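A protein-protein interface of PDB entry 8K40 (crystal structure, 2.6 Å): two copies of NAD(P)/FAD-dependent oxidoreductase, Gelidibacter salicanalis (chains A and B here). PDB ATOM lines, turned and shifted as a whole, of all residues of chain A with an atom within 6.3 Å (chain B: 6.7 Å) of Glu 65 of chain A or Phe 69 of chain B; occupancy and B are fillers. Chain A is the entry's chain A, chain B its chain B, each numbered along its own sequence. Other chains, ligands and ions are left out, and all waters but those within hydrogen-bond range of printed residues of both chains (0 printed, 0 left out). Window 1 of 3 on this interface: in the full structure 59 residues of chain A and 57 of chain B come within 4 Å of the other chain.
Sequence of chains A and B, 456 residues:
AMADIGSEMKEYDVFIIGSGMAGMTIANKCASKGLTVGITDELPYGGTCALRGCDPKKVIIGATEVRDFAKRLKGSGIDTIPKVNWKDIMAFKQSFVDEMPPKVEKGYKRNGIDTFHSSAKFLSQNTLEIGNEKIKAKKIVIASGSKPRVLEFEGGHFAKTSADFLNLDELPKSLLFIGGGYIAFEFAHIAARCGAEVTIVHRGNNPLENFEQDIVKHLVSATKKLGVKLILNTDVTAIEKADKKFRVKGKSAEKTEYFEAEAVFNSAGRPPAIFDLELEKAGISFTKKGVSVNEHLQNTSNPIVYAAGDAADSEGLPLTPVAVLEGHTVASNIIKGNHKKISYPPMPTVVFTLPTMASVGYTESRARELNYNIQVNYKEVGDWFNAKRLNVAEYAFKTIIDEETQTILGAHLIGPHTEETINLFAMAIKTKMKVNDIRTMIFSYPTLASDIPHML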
ATOM      1  N   LYS A  58     -15.438   8.923 -26.498  1.00  0.00           N
ATOM      2  CA  LYS A  58     -14.360   8.304 -25.674  1.00  0.00           C
ATOM      3  C   LYS A  58     -14.782   6.884 -25.248  1.00  0.00           C
ATOM      4  O   LYS A  58     -13.914   5.964 -25.302  1.00  0.00           O
ATOM      5  CB  LYS A  58     -13.995   9.211 -24.494  1.00  0.00           C
ATOM      6  CG  LYS A  58     -12.632   8.958 -23.852  1.00  0.00           C
ATOM      7  CD  LYS A  58     -11.440   9.069 -24.789  1.00  0.00           C
ATOM      8  CE  LYS A  58     -10.114   8.746 -24.126  1.00  0.00           C
ATOM      9  NZ  LYS A  58      -9.298   7.843 -24.974  1.00  0.00           N
ATOM     10  N   ILE A  60     -16.881   4.723 -26.924  1.00  0.00           N
ATOM     11  CA  ILE A  60     -16.653   3.953 -28.180  1.00  0.00           C
ATOM     12  C   ILE A  60     -15.161   3.669 -28.399  1.00  0.00           C
ATOM     13  O   ILE A  60     -14.830   2.524 -28.768  1.00  0.00           O
ATOM     14  CB  ILE A  60     -17.231   4.696 -29.390  1.00  0.00           C
ATOM     15  CG1 ILE A  60     -18.751   4.855 -29.258  1.00  0.00           C
ATOM     16  CG2 ILE A  60     -16.802   3.980 -30.667  1.00  0.00           C
ATOM     17  CD1 ILE A  60     -19.450   5.382 -30.500  1.00  0.00           C
ATOM     18  N   ILE A  61     -14.302   4.684 -28.268  1.00  0.00           N
ATOM     19  CA  ILE A  61     -12.834   4.555 -28.523  1.00  0.00           C
ATOM     20  C   ILE A  61     -12.242   3.482 -27.598  1.00  0.00           C
ATOM     21  O   ILE A  61     -11.399   2.724 -28.067  1.00  0.00           O
ATOM     22  CB  ILE A  61     -12.149   5.923 -28.394  1.00  0.00           C
ATOM     23  CG1 ILE A  61     -12.413   6.740 -29.658  1.00  0.00           C
ATOM     24  CG2 ILE A  61     -10.652   5.801 -28.096  1.00  0.00           C
ATOM     25  CD1 ILE A  61     -12.337   8.204 -29.441  1.00  0.00           C
ATOM     26  N   GLY A  62     -12.717   3.385 -26.355  1.00  0.00           N
ATOM     27  CA  GLY A  62     -12.464   2.250 -25.444  1.00  0.00           C
ATOM     28  C   GLY A  62     -12.224   0.928 -26.164  1.00  0.00           C
ATOM     29  O   GLY A  62     -11.106   0.374 -26.014  1.00  0.00           O
ATOM     30  N   ALA A  63     -13.221   0.404 -26.885  1.00  0.00           N
ATOM     31  CA  ALA A  63     -13.183  -0.960 -27.480  1.00  0.00           C
ATOM     32  C   ALA A  63     -12.152  -1.038 -28.608  1.00  0.00           C
ATOM     33  O   ALA A  63     -11.558  -2.121 -28.804  1.00  0.00           O
ATOM     34  CB  ALA A  63     -14.540  -1.371 -27.989  1.00  0.00           C
ATOM     35  N   THR A  64     -11.982   0.045 -29.361  1.00  0.00           N
ATOM     36  CA  THR A  64     -10.959   0.112 -30.431  1.00  0.00           C
ATOM     37  C   THR A  64      -9.575   0.006 -29.779  1.00  0.00           C
ATOM     38  O   THR A  64      -8.694  -0.588 -30.413  1.00  0.00           O
ATOM     39  CB  THR A  64     -11.104   1.353 -31.335  1.00  0.00           C
ATOM     40  OG1 THR A  64     -10.711   2.547 -30.649  1.00  0.00           O
ATOM     41  CG2 THR A  64     -12.502   1.528 -31.888  1.00  0.00           C
ATOM     42  N   GLU A  65      -9.364   0.559 -28.579  1.00  0.00           N
ATOM     43  CA  GLU A  65      -8.001   0.587 -27.957  1.00  0.00           C
ATOM     44  C   GLU A  65      -7.614  -0.856 -27.680  1.00  0.00           C
ATOM     45  O   GLU A  65      -6.480  -1.245 -27.975  1.00  0.00           O
ATOM     46  CB  GLU A  65      -7.895   1.386 -26.653  1.00  0.00           C
ATOM     47  CG  GLU A  65      -8.456   2.781 -26.756  1.00  0.00           C
ATOM     48  CD  GLU A  65      -8.201   3.665 -25.555  1.00  0.00           C
ATOM     49  OE1 GLU A  65      -7.070   4.165 -25.442  1.00  0.00           O
ATOM     50  OE2 GLU A  65      -9.135   3.849 -24.737  1.00  0.00           O
ATOM     51  N   VAL A  66      -8.570  -1.614 -27.166  1.00  0.00           N
ATOM     52  CA  VAL A  66      -8.396  -3.064 -26.907  1.00  0.00           C
ATOM     53  C   VAL A  66      -7.948  -3.709 -28.208  1.00  0.00           C
ATOM     54  O   VAL A  66      -6.947  -4.416 -28.175  1.00  0.00           O
ATOM     55  CB  VAL A  66      -9.683  -3.725 -26.399  1.00  0.00           C
ATOM     56  CG1 VAL A  66      -9.498  -5.238 -26.287  1.00  0.00           C
ATOM     57  CG2 VAL A  66     -10.135  -3.110 -25.083  1.00  0.00           C
ATOM     58  N   ARG A  67      -8.701  -3.501 -29.285  1.00  0.00           N
ATOM     59  CA  ARG A  67      -8.369  -4.109 -30.591  1.00  0.00           C
ATOM     60  C   ARG A  67      -6.962  -3.657 -30.983  1.00  0.00           C
ATOM     61  O   ARG A  67      -6.126  -4.539 -31.268  1.00  0.00           O
ATOM     62  CB  ARG A  67      -9.400  -3.729 -31.654  1.00  0.00           C
ATOM     63  CG  ARG A  67      -8.999  -4.139 -33.062  1.00  0.00           C
ATOM     64  CD  ARG A  67     -10.109  -3.962 -34.079  1.00  0.00           C
ATOM     65  NE  ARG A  67      -9.622  -4.468 -35.356  1.00  0.00           N
ATOM     66  CZ  ARG A  67      -9.688  -5.738 -35.766  1.00  0.00           C
ATOM     67  NH1 ARG A  67     -10.273  -6.667 -35.027  1.00  0.00           N
ATOM     68  NH2 ARG A  67      -9.178  -6.070 -36.938  1.00  0.00           N
ATOM     69  N   ASP A  68      -6.709  -2.341 -30.993  1.00  0.00           N
ATOM     70  CA  ASP A  68      -5.419  -1.745 -31.449  1.00  0.00           C
ATOM     71  C   ASP A  68      -4.276  -2.373 -30.642  1.00  0.00           C
ATOM     72  O   ASP A  68      -3.257  -2.783 -31.237  1.00  0.00           O
ATOM     73  CB  ASP A  68      -5.400  -0.218 -31.310  1.00  0.00           C
ATOM     74  CG  ASP A  68      -4.223   0.439 -32.021  1.00  0.00           C
ATOM     75  OD1 ASP A  68      -4.200   0.418 -33.282  1.00  0.00           O
ATOM     76  OD2 ASP A  68      -3.321   0.942 -31.317  1.00  0.00           O
ATOM     77  N   PHE A  69      -4.448  -2.475 -29.323  1.00  0.00           N
ATOM     78  CA  PHE A  69      -3.420  -3.024 -28.400  1.00  0.00           C
ATOM     79  C   PHE A  69      -3.121  -4.500 -28.748  1.00  0.00           C
ATOM     80  O   PHE A  69      -1.942  -4.866 -28.985  1.00  0.00           O
ATOM     81  CB  PHE A  69      -3.882  -2.811 -26.957  1.00  0.00           C
ATOM     82  CG  PHE A  69      -2.792  -2.726 -25.922  1.00  0.00           C
ATOM     83  CD1 PHE A  69      -1.465  -2.983 -26.243  1.00  0.00           C
ATOM     84  CD2 PHE A  69      -3.118  -2.429 -24.604  1.00  0.00           C
ATOM     85  CE1 PHE A  69      -0.482  -2.901 -25.271  1.00  0.00           C
ATOM     86  CE2 PHE A  69      -2.134  -2.358 -23.630  1.00  0.00           C
ATOM     87  CZ  PHE A  69      -0.815  -2.574 -23.973  1.00  0.00           C
ATOM     88  N   ALA A  70      -4.148  -5.350 -28.817  1.00  0.00           N
ATOM     89  CA  ALA A  70      -4.012  -6.771 -29.230  1.00  0.00           C
ATOM     90  C   ALA A  70      -3.295  -6.853 -30.580  1.00  0.00           C
ATOM     91  O   ALA A  70      -2.401  -7.700 -30.725  1.00  0.00           O
ATOM     92  CB  ALA A  70      -5.356  -7.447 -29.301  1.00  0.00           C
ATOM     93  N   ARG A  72      -1.159  -4.718 -31.899  1.00  0.00           N
ATOM     94  CA  ARG A  72       0.260  -4.285 -31.766  1.00  0.00           C
ATOM     95  C   ARG A  72       1.127  -5.425 -31.183  1.00  0.00           C
ATOM     96  O   ARG A  72       2.292  -5.541 -31.583  1.00  0.00           O
ATOM     97  CB  ARG A  72       0.318  -2.972 -30.964  1.00  0.00           C
ATOM     98  CG  ARG A  72       0.022  -1.730 -31.802  1.00  0.00           C
ATOM     99  CD  ARG A  72       0.105  -0.390 -31.078  1.00  0.00           C
ATOM    100  NE  ARG A  72      -1.101  -0.156 -30.285  1.00  0.00           N
ATOM    101  CZ  ARG A  72      -1.184  -0.133 -28.947  1.00  0.00           C
ATOM    102  NH1 ARG A  72      -0.112  -0.290 -28.181  1.00  0.00           N
ATOM    103  NH2 ARG A  72      -2.360   0.071 -28.373  1.00  0.00           N
ATOM    104  N   ARG A 193     -11.160   0.825 -37.583  1.00  0.00           N
ATOM    105  CA  ARG A 193     -10.828  -0.196 -36.559  1.00  0.00           C
ATOM    106  C   ARG A 193     -12.023  -1.139 -36.379  1.00  0.00           C
ATOM    107  O   ARG A 193     -11.793  -2.322 -36.081  1.00  0.00           O
ATOM    108  CB  ARG A 193     -10.377   0.475 -35.260  1.00  0.00           C
ATOM    109  CG  ARG A 193      -8.959   1.019 -35.352  1.00  0.00           C
ATOM    110  CD  ARG A 193      -8.228   1.143 -34.031  1.00  0.00           C
ATOM    111  NE  ARG A 193      -6.918   1.715 -34.294  1.00  0.00           N
ATOM    112  CZ  ARG A 193      -6.673   3.015 -34.438  1.00  0.00           C
ATOM    113  NH1 ARG A 193      -7.636   3.922 -34.305  1.00  0.00           N
ATOM    114  NH2 ARG A 193      -5.439   3.413 -34.670  1.00  0.00           N
ATOM    115  N   LEU A 354      -5.768   6.974 -32.523  1.00  0.00           N
ATOM    116  CA  LEU A 354      -4.678   6.110 -32.011  1.00  0.00           C
ATOM    117  C   LEU A 354      -3.626   6.051 -33.106  1.00  0.00           C
ATOM    118  O   LEU A 354      -3.932   5.570 -34.187  1.00  0.00           O
ATOM    119  CB  LEU A 354      -5.234   4.720 -31.679  1.00  0.00           C
ATOM    120  CG  LEU A 354      -6.423   4.696 -30.723  1.00  0.00           C
ATOM    121  CD1 LEU A 354      -6.975   3.291 -30.586  1.00  0.00           C
ATOM    122  CD2 LEU A 354      -6.023   5.242 -29.360  1.00  0.00           C
ATOM    123  N   GLU A 419      -2.495  12.282 -24.548  1.00  0.00           N
ATOM    124  CA  GLU A 419      -3.690  12.950 -23.956  1.00  0.00           C
ATOM    125  C   GLU A 419      -3.489  13.220 -22.458  1.00  0.00           C
ATOM    126  O   GLU A 419      -4.025  14.239 -21.989  1.00  0.00           O
ATOM    127  CB  GLU A 419      -4.980  12.174 -24.219  1.00  0.00           C
ATOM    128  CG  GLU A 419      -5.173  10.926 -23.396  1.00  0.00           C
ATOM    129  CD  GLU A 419      -4.488   9.677 -23.906  1.00  0.00           C
ATOM    130  OE1 GLU A 419      -3.562   9.803 -24.729  1.00  0.00           O
ATOM    131  OE2 GLU A 419      -4.860   8.580 -23.442  1.00  0.00           O
ATOM    132  N   THR B  64      -0.607  -8.446 -20.474  1.00  0.00           N
ATOM    133  CA  THR B  64      -1.645  -8.681 -19.446  1.00  0.00           C
ATOM    134  C   THR B  64      -2.658  -7.539 -19.509  1.00  0.00           C
ATOM    135  O   THR B  64      -3.844  -7.855 -19.330  1.00  0.00           O
ATOM    136  CB  THR B  64      -1.040  -8.909 -18.050  1.00  0.00           C
ATOM    137  OG1 THR B  64      -0.632  -7.654 -17.498  1.00  0.00           O
ATOM    138  CG2 THR B  64       0.104  -9.907 -18.068  1.00  0.00           C
ATOM    139  N   GLU B  65      -2.211  -6.290 -19.752  1.00  0.00           N
ATOM    140  CA  GLU B  65      -3.087  -5.090 -19.907  1.00  0.00           C
ATOM    141  C   GLU B  65      -4.071  -5.386 -21.048  1.00  0.00           C
ATOM    142  O   GLU B  65      -5.256  -5.071 -20.855  1.00  0.00           O
ATOM    143  CB  GLU B  65      -2.362  -3.766 -20.233  1.00  0.00           C
ATOM    144  CG  GLU B  65      -1.072  -3.502 -19.458  1.00  0.00           C
ATOM    145  CD  GLU B  65      -0.487  -2.092 -19.519  1.00  0.00           C
ATOM    146  OE1 GLU B  65      -0.926  -1.233 -18.710  1.00  0.00           O
ATOM    147  OE2 GLU B  65       0.441  -1.858 -20.342  1.00  0.00           O
ATOM    148  N   VAL B  66      -3.618  -5.984 -22.169  1.00  0.00           N
ATOM    149  CA  VAL B  66      -4.534  -6.356 -23.292  1.00  0.00           C
ATOM    150  C   VAL B  66      -5.625  -7.271 -22.726  1.00  0.00           C
ATOM    151  O   VAL B  66      -6.829  -6.981 -22.906  1.00  0.00           O
ATOM    152  CB  VAL B  66      -3.855  -7.066 -24.479  1.00  0.00           C
ATOM    153  CG1 VAL B  66      -4.904  -7.404 -25.520  1.00  0.00           C
ATOM    154  CG2 VAL B  66      -2.728  -6.272 -25.127  1.00  0.00           C
ATOM    155  N   ARG B  67      -5.217  -8.373 -22.102  1.00  0.00           N
ATOM    156  CA  ARG B  67      -6.162  -9.382 -21.568  1.00  0.00           C
ATOM    157  C   ARG B  67      -7.121  -8.677 -20.610  1.00  0.00           C
ATOM    158  O   ARG B  67      -8.341  -8.818 -20.791  1.00  0.00           O
ATOM    159  CB  ARG B  67      -5.407 -10.532 -20.897  1.00  0.00           C
ATOM    160  CG  ARG B  67      -6.314 -11.458 -20.108  1.00  0.00           C
ATOM    161  CD  ARG B  67      -5.617 -12.657 -19.502  1.00  0.00           C
ATOM    162  NE  ARG B  67      -6.647 -13.447 -18.855  1.00  0.00           N
ATOM    163  CZ  ARG B  67      -7.441 -14.299 -19.491  1.00  0.00           C
ATOM    164  NH1 ARG B  67      -7.293 -14.529 -20.788  1.00  0.00           N
ATOM    165  NH2 ARG B  67      -8.382 -14.922 -18.813  1.00  0.00           N
ATOM    166  N   ASP B  68      -6.584  -7.942 -19.635  1.00  0.00           N
ATOM    167  CA  ASP B  68      -7.376  -7.217 -18.602  1.00  0.00           C
ATOM    168  C   ASP B  68      -8.406  -6.307 -19.280  1.00  0.00           C
ATOM    169  O   ASP B  68      -9.589  -6.343 -18.873  1.00  0.00           O
ATOM    170  CB  ASP B  68      -6.467  -6.405 -17.677  1.00  0.00           C
ATOM    171  CG  ASP B  68      -7.190  -5.775 -16.495  1.00  0.00           C
ATOM    172  OD1 ASP B  68      -7.625  -6.532 -15.614  1.00  0.00           O
ATOM    173  OD2 ASP B  68      -7.308  -4.529 -16.463  1.00  0.00           O
ATOM    174  N   PHE B  69      -7.972  -5.504 -20.262  1.00  0.00           N
ATOM    175  CA  PHE B  69      -8.816  -4.479 -20.932  1.00  0.00           C
ATOM    176  C   PHE B  69      -9.916  -5.222 -21.704  1.00  0.00           C
ATOM    177  O   PHE B  69     -11.106  -4.910 -21.515  1.00  0.00           O
ATOM    178  CB  PHE B  69      -7.946  -3.549 -21.786  1.00  0.00           C
ATOM    179  CG  PHE B  69      -8.528  -2.203 -22.142  1.00  0.00           C
ATOM    180  CD1 PHE B  69      -9.861  -1.893 -21.904  1.00  0.00           C
ATOM    181  CD2 PHE B  69      -7.731  -1.241 -22.760  1.00  0.00           C
ATOM    182  CE1 PHE B  69     -10.380  -0.655 -22.265  1.00  0.00           C
ATOM    183  CE2 PHE B  69      -8.247  -0.001 -23.114  1.00  0.00           C
ATOM    184  CZ  PHE B  69      -9.573   0.288 -22.875  1.00  0.00           C
ATOM    185  N   ALA B  70      -9.528  -6.225 -22.493  1.00  0.00           N
ATOM    186  CA  ALA B  70     -10.438  -7.124 -23.236  1.00  0.00           C
ATOM    187  C   ALA B  70     -11.097  -8.047 -22.230  1.00  0.00           C
ATOM    188  O   ALA B  70     -10.719  -9.214 -22.214  1.00  0.00           O
ATOM    189  CB  ALA B  70      -9.677  -7.945 -24.246  1.00  0.00           C
ATOM    190  N   LYS B  71     -12.012  -7.550 -21.413  1.00  0.00           N
ATOM    191  CA  LYS B  71     -12.613  -8.348 -20.307  1.00  0.00           C
ATOM    192  C   LYS B  71     -13.354  -7.395 -19.378  1.00  0.00           C
ATOM    193  O   LYS B  71     -14.460  -7.739 -18.892  1.00  0.00           O
ATOM    194  CB  LYS B  71     -11.562  -9.132 -19.511  1.00  0.00           C
ATOM    195  CG  LYS B  71     -12.043  -9.694 -18.174  1.00  0.00           C
ATOM    196  CD  LYS B  71     -10.919 -10.099 -17.232  1.00  0.00           C
ATOM    197  CE  LYS B  71     -11.193  -9.750 -15.783  1.00  0.00           C
ATOM    198  NZ  LYS B  71      -9.937  -9.684 -14.994  1.00  0.00           N
ATOM    199  N   ARG B  72     -12.761  -6.234 -19.141  1.00  0.00           N
ATOM    200  CA  ARG B  72     -13.524  -5.102 -18.585  1.00  0.00           C
ATOM    201  C   ARG B  72     -14.628  -4.746 -19.595  1.00  0.00           C
ATOM    202  O   ARG B  72     -15.744  -4.402 -19.160  1.00  0.00           O
ATOM    203  CB  ARG B  72     -12.546  -3.988 -18.205  1.00  0.00           C
ATOM    204  CG  ARG B  72     -11.719  -4.336 -16.975  1.00  0.00           C
ATOM    205  CD  ARG B  72     -10.903  -3.186 -16.420  1.00  0.00           C
ATOM    206  NE  ARG B  72      -9.619  -3.100 -17.108  1.00  0.00           N
ATOM    207  CZ  ARG B  72      -9.292  -2.201 -18.025  1.00  0.00           C
ATOM    208  NH1 ARG B  72     -10.145  -1.257 -18.402  1.00  0.00           N
ATOM    209  NH2 ARG B  72      -8.087  -2.248 -18.553  1.00  0.00           N
ATOM    210  N   LEU B  73     -14.357  -4.877 -20.893  1.00  0.00           N
ATOM    211  CA  LEU B  73     -15.334  -4.500 -21.942  1.00  0.00           C
ATOM    212  C   LEU B  73     -15.957  -5.767 -22.523  1.00  0.00           C
ATOM    213  O   LEU B  73     -16.656  -5.658 -23.545  1.00  0.00           O
ATOM    214  CB  LEU B  73     -14.640  -3.639 -23.003  1.00  0.00           C
ATOM    215  CG  LEU B  73     -14.162  -2.275 -22.499  1.00  0.00           C
ATOM    216  CD1 LEU B  73     -13.616  -1.427 -23.632  1.00  0.00           C
ATOM    217  CD2 LEU B  73     -15.270  -1.539 -21.775  1.00  0.00           C
ATOM    218  N   LYS B  74     -15.723  -6.913 -21.881  1.00  0.00           N
ATOM    219  CA  LYS B  74     -16.410  -8.190 -22.202  1.00  0.00           C
ATOM    220  C   LYS B  74     -17.919  -7.925 -22.148  1.00  0.00           C
ATOM    221  O   LYS B  74     -18.392  -7.400 -21.093  1.00  0.00           O
ATOM    222  CB  LYS B  74     -15.985  -9.299 -21.234  1.00  0.00           C
ATOM    223  CG  LYS B  74     -16.805 -10.580 -21.265  1.00  0.00           C
ATOM    224  CD  LYS B  74     -16.585 -11.425 -22.490  1.00  0.00           C
ATOM    225  CE  LYS B  74     -17.688 -12.449 -22.652  1.00  0.00           C
ATOM    226  NZ  LYS B  74     -17.498 -13.276 -23.865  1.00  0.00           N
ATOM    227  N   ILE B  78     -16.540  -5.968 -26.554  1.00  0.00           N
ATOM    228  CA  ILE B  78     -15.526  -7.046 -26.744  1.00  0.00           C
ATOM    229  C   ILE B  78     -16.201  -8.378 -26.397  1.00  0.00           C
ATOM    230  O   ILE B  78     -16.918  -8.459 -25.353  1.00  0.00           O
ATOM    231  CB  ILE B  78     -14.244  -6.756 -25.936  1.00  0.00           C
ATOM    232  CG1 ILE B  78     -13.659  -5.393 -26.319  1.00  0.00           C
ATOM    233  CG2 ILE B  78     -13.208  -7.863 -26.100  1.00  0.00           C
ATOM    234  CD1 ILE B  78     -13.024  -5.371 -27.704  1.00  0.00           C
ATOM    235  N   LEU B 354      -2.621  -4.239 -11.860  1.00  0.00           N
ATOM    236  CA  LEU B 354      -3.849  -3.675 -12.478  1.00  0.00           C
ATOM    237  C   LEU B 354      -5.026  -3.863 -11.535  1.00  0.00           C
ATOM    238  O   LEU B 354      -5.377  -4.986 -11.201  1.00  0.00           O
ATOM    239  CB  LEU B 354      -4.108  -4.362 -13.811  1.00  0.00           C
ATOM    240  CG  LEU B 354      -2.971  -4.253 -14.814  1.00  0.00           C
ATOM    241  CD1 LEU B 354      -3.281  -5.114 -16.029  1.00  0.00           C
ATOM    242  CD2 LEU B 354      -2.739  -2.798 -15.206  1.00  0.00           C
ATOM    243  N   ARG B 389     -16.326   4.061 -17.571  1.00  0.00           N
ATOM    244  CA  ARG B 389     -16.286   3.867 -19.045  1.00  0.00           C
ATOM    245  C   ARG B 389     -15.298   2.758 -19.375  1.00  0.00           C
ATOM    246  O   ARG B 389     -15.485   2.159 -20.417  1.00  0.00           O
ATOM    247  CB  ARG B 389     -15.929   5.153 -19.784  1.00  0.00           C
ATOM    248  CG  ARG B 389     -14.526   5.684 -19.523  1.00  0.00           C
ATOM    249  CD  ARG B 389     -14.311   7.068 -20.132  1.00  0.00           C
ATOM    250  NE  ARG B 389     -13.023   7.630 -19.741  1.00  0.00           N
ATOM    251  CZ  ARG B 389     -11.839   7.205 -20.173  1.00  0.00           C
ATOM    252  NH1 ARG B 389     -11.759   6.208 -21.032  1.00  0.00           N
ATOM    253  NH2 ARG B 389     -10.730   7.777 -19.739  1.00  0.00           N
ATOM    254  N   LEU B 390     -14.337   2.500 -18.480  1.00  0.00           N
ATOM    255  CA  LEU B 390     -13.270   1.467 -18.594  1.00  0.00           C
ATOM    256  C   LEU B 390     -13.684   0.198 -17.838  1.00  0.00           C
ATOM    257  O   LEU B 390     -12.911  -0.802 -17.876  1.00  0.00           O
ATOM    258  CB  LEU B 390     -11.967   2.054 -18.025  1.00  0.00           C
ATOM    259  CG  LEU B 390     -11.380   3.182 -18.867  1.00  0.00           C
ATOM    260  CD1 LEU B 390     -10.049   3.671 -18.323  1.00  0.00           C
ATOM    261  CD2 LEU B 390     -11.228   2.739 -20.311  1.00  0.00           C
ATOM    262  N   HIS B 417      -4.506   4.707 -14.995  1.00  0.00           N
ATOM    263  CA  HIS B 417      -3.423   5.658 -15.362  1.00  0.00           C
ATOM    264  C   HIS B 417      -2.729   6.266 -14.138  1.00  0.00           C
ATOM    265  O   HIS B 417      -2.038   7.257 -14.308  1.00  0.00           O
ATOM    266  CB  HIS B 417      -3.947   6.703 -16.355  1.00  0.00           C
ATOM    267  CG  HIS B 417      -4.557   6.064 -17.557  1.00  0.00           C
ATOM    268  ND1 HIS B 417      -4.114   4.853 -18.037  1.00  0.00           N
ATOM    269  CD2 HIS B 417      -5.597   6.421 -18.339  1.00  0.00           C
ATOM    270  CE1 HIS B 417      -4.850   4.496 -19.070  1.00  0.00           C
ATOM    271  NE2 HIS B 417      -5.773   5.433 -19.267  1.00  0.00           N
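Glu 65 of chain A touches Phe 69 of chain B, and with the chains exchanged Phe 69 of chain A touches Glu 65 of chain B. Val 66 of chain A touches Phe 69 of chain B, and with the chains exchanged Phe 69 of chain A touches Val 66 of chain B. Val 66 of chain A touches Ala 70 of chain B, and with the chains exchanged Ala 70 of chain A touches Val 66 of chain B. Positions printed for both chains: 64, 65, 66, 67, 68, 69, 70, 72 and 354. Of the 11 pairs that touch across the chains among the printed residues, 6 have their exchanged pair printed and touching as well.
CZ of Phe 69 of chain B touches O of Gly 62 of chain A, 3.5 Å away. Leu 73 of chain B touches Gly 62 of chain A. Leu 73 of chain B touches Ala 63 of chain A. Ile 78 of chain B touches Ala 63 of chain A (CD1 to O, 3.7 Å). CE2 of Phe 69 of chain B touches CB of Glu 65 of chain A, at 3.8 Å. Val 66 of chain A touches Ala 70 of chain B (CG1 to CB, 3.4 Å). Ile 78 of chain B touches Val 66 of chain A (CD1 to CG1, 3.8 Å). Phe 69 of chain A touches Glu 65 of chain B (CE2 to CB, 3.7 Å). CG of Phe 69 of chain A touches CG2 of Val 66 of chain B (3.6 Å). Ala 70 of chain A touches Val 66 of chain B (CB to CG1, 3.8 Å).
N of Ile 78 of chain B sits at hydrogen-bond distance from O of Leu 73 of chain B (3.0 Å).
Hydrophobic or aromatic side chains of chain A that line the printed part of chain B: Val 66, Phe 69 and Ala 70. Along chain A the printed residues that touch a printed residue of chain B span positions 62 to 70. Hydrophobic or aromatic side chains of chain B within 4 Å of the printed part of chain A: Val 66, Phe 69, Ala 70, Leu 73 and Ile 78. Among the printed residues, 11 pairs touch across the chains.
Of the printed residues of chain A, Phe 69 of chain B touches Gly 62 (3.5 Å), Glu 65 (3.8 Å) and Val 66 (3.4 Å). Printed residues of chain A within 4 Å of Ile 78 of chain B: Ala 63 (3.7 Å) and Val 66 (3.8 Å). Printed residues of chain A within 4 Å of Leu 73 of chain B: Gly 62 and Ala 63. The nearest residue of chain A that does not touch Phe 69 of chain B is Phe 69 of chain A (5.1 Å).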
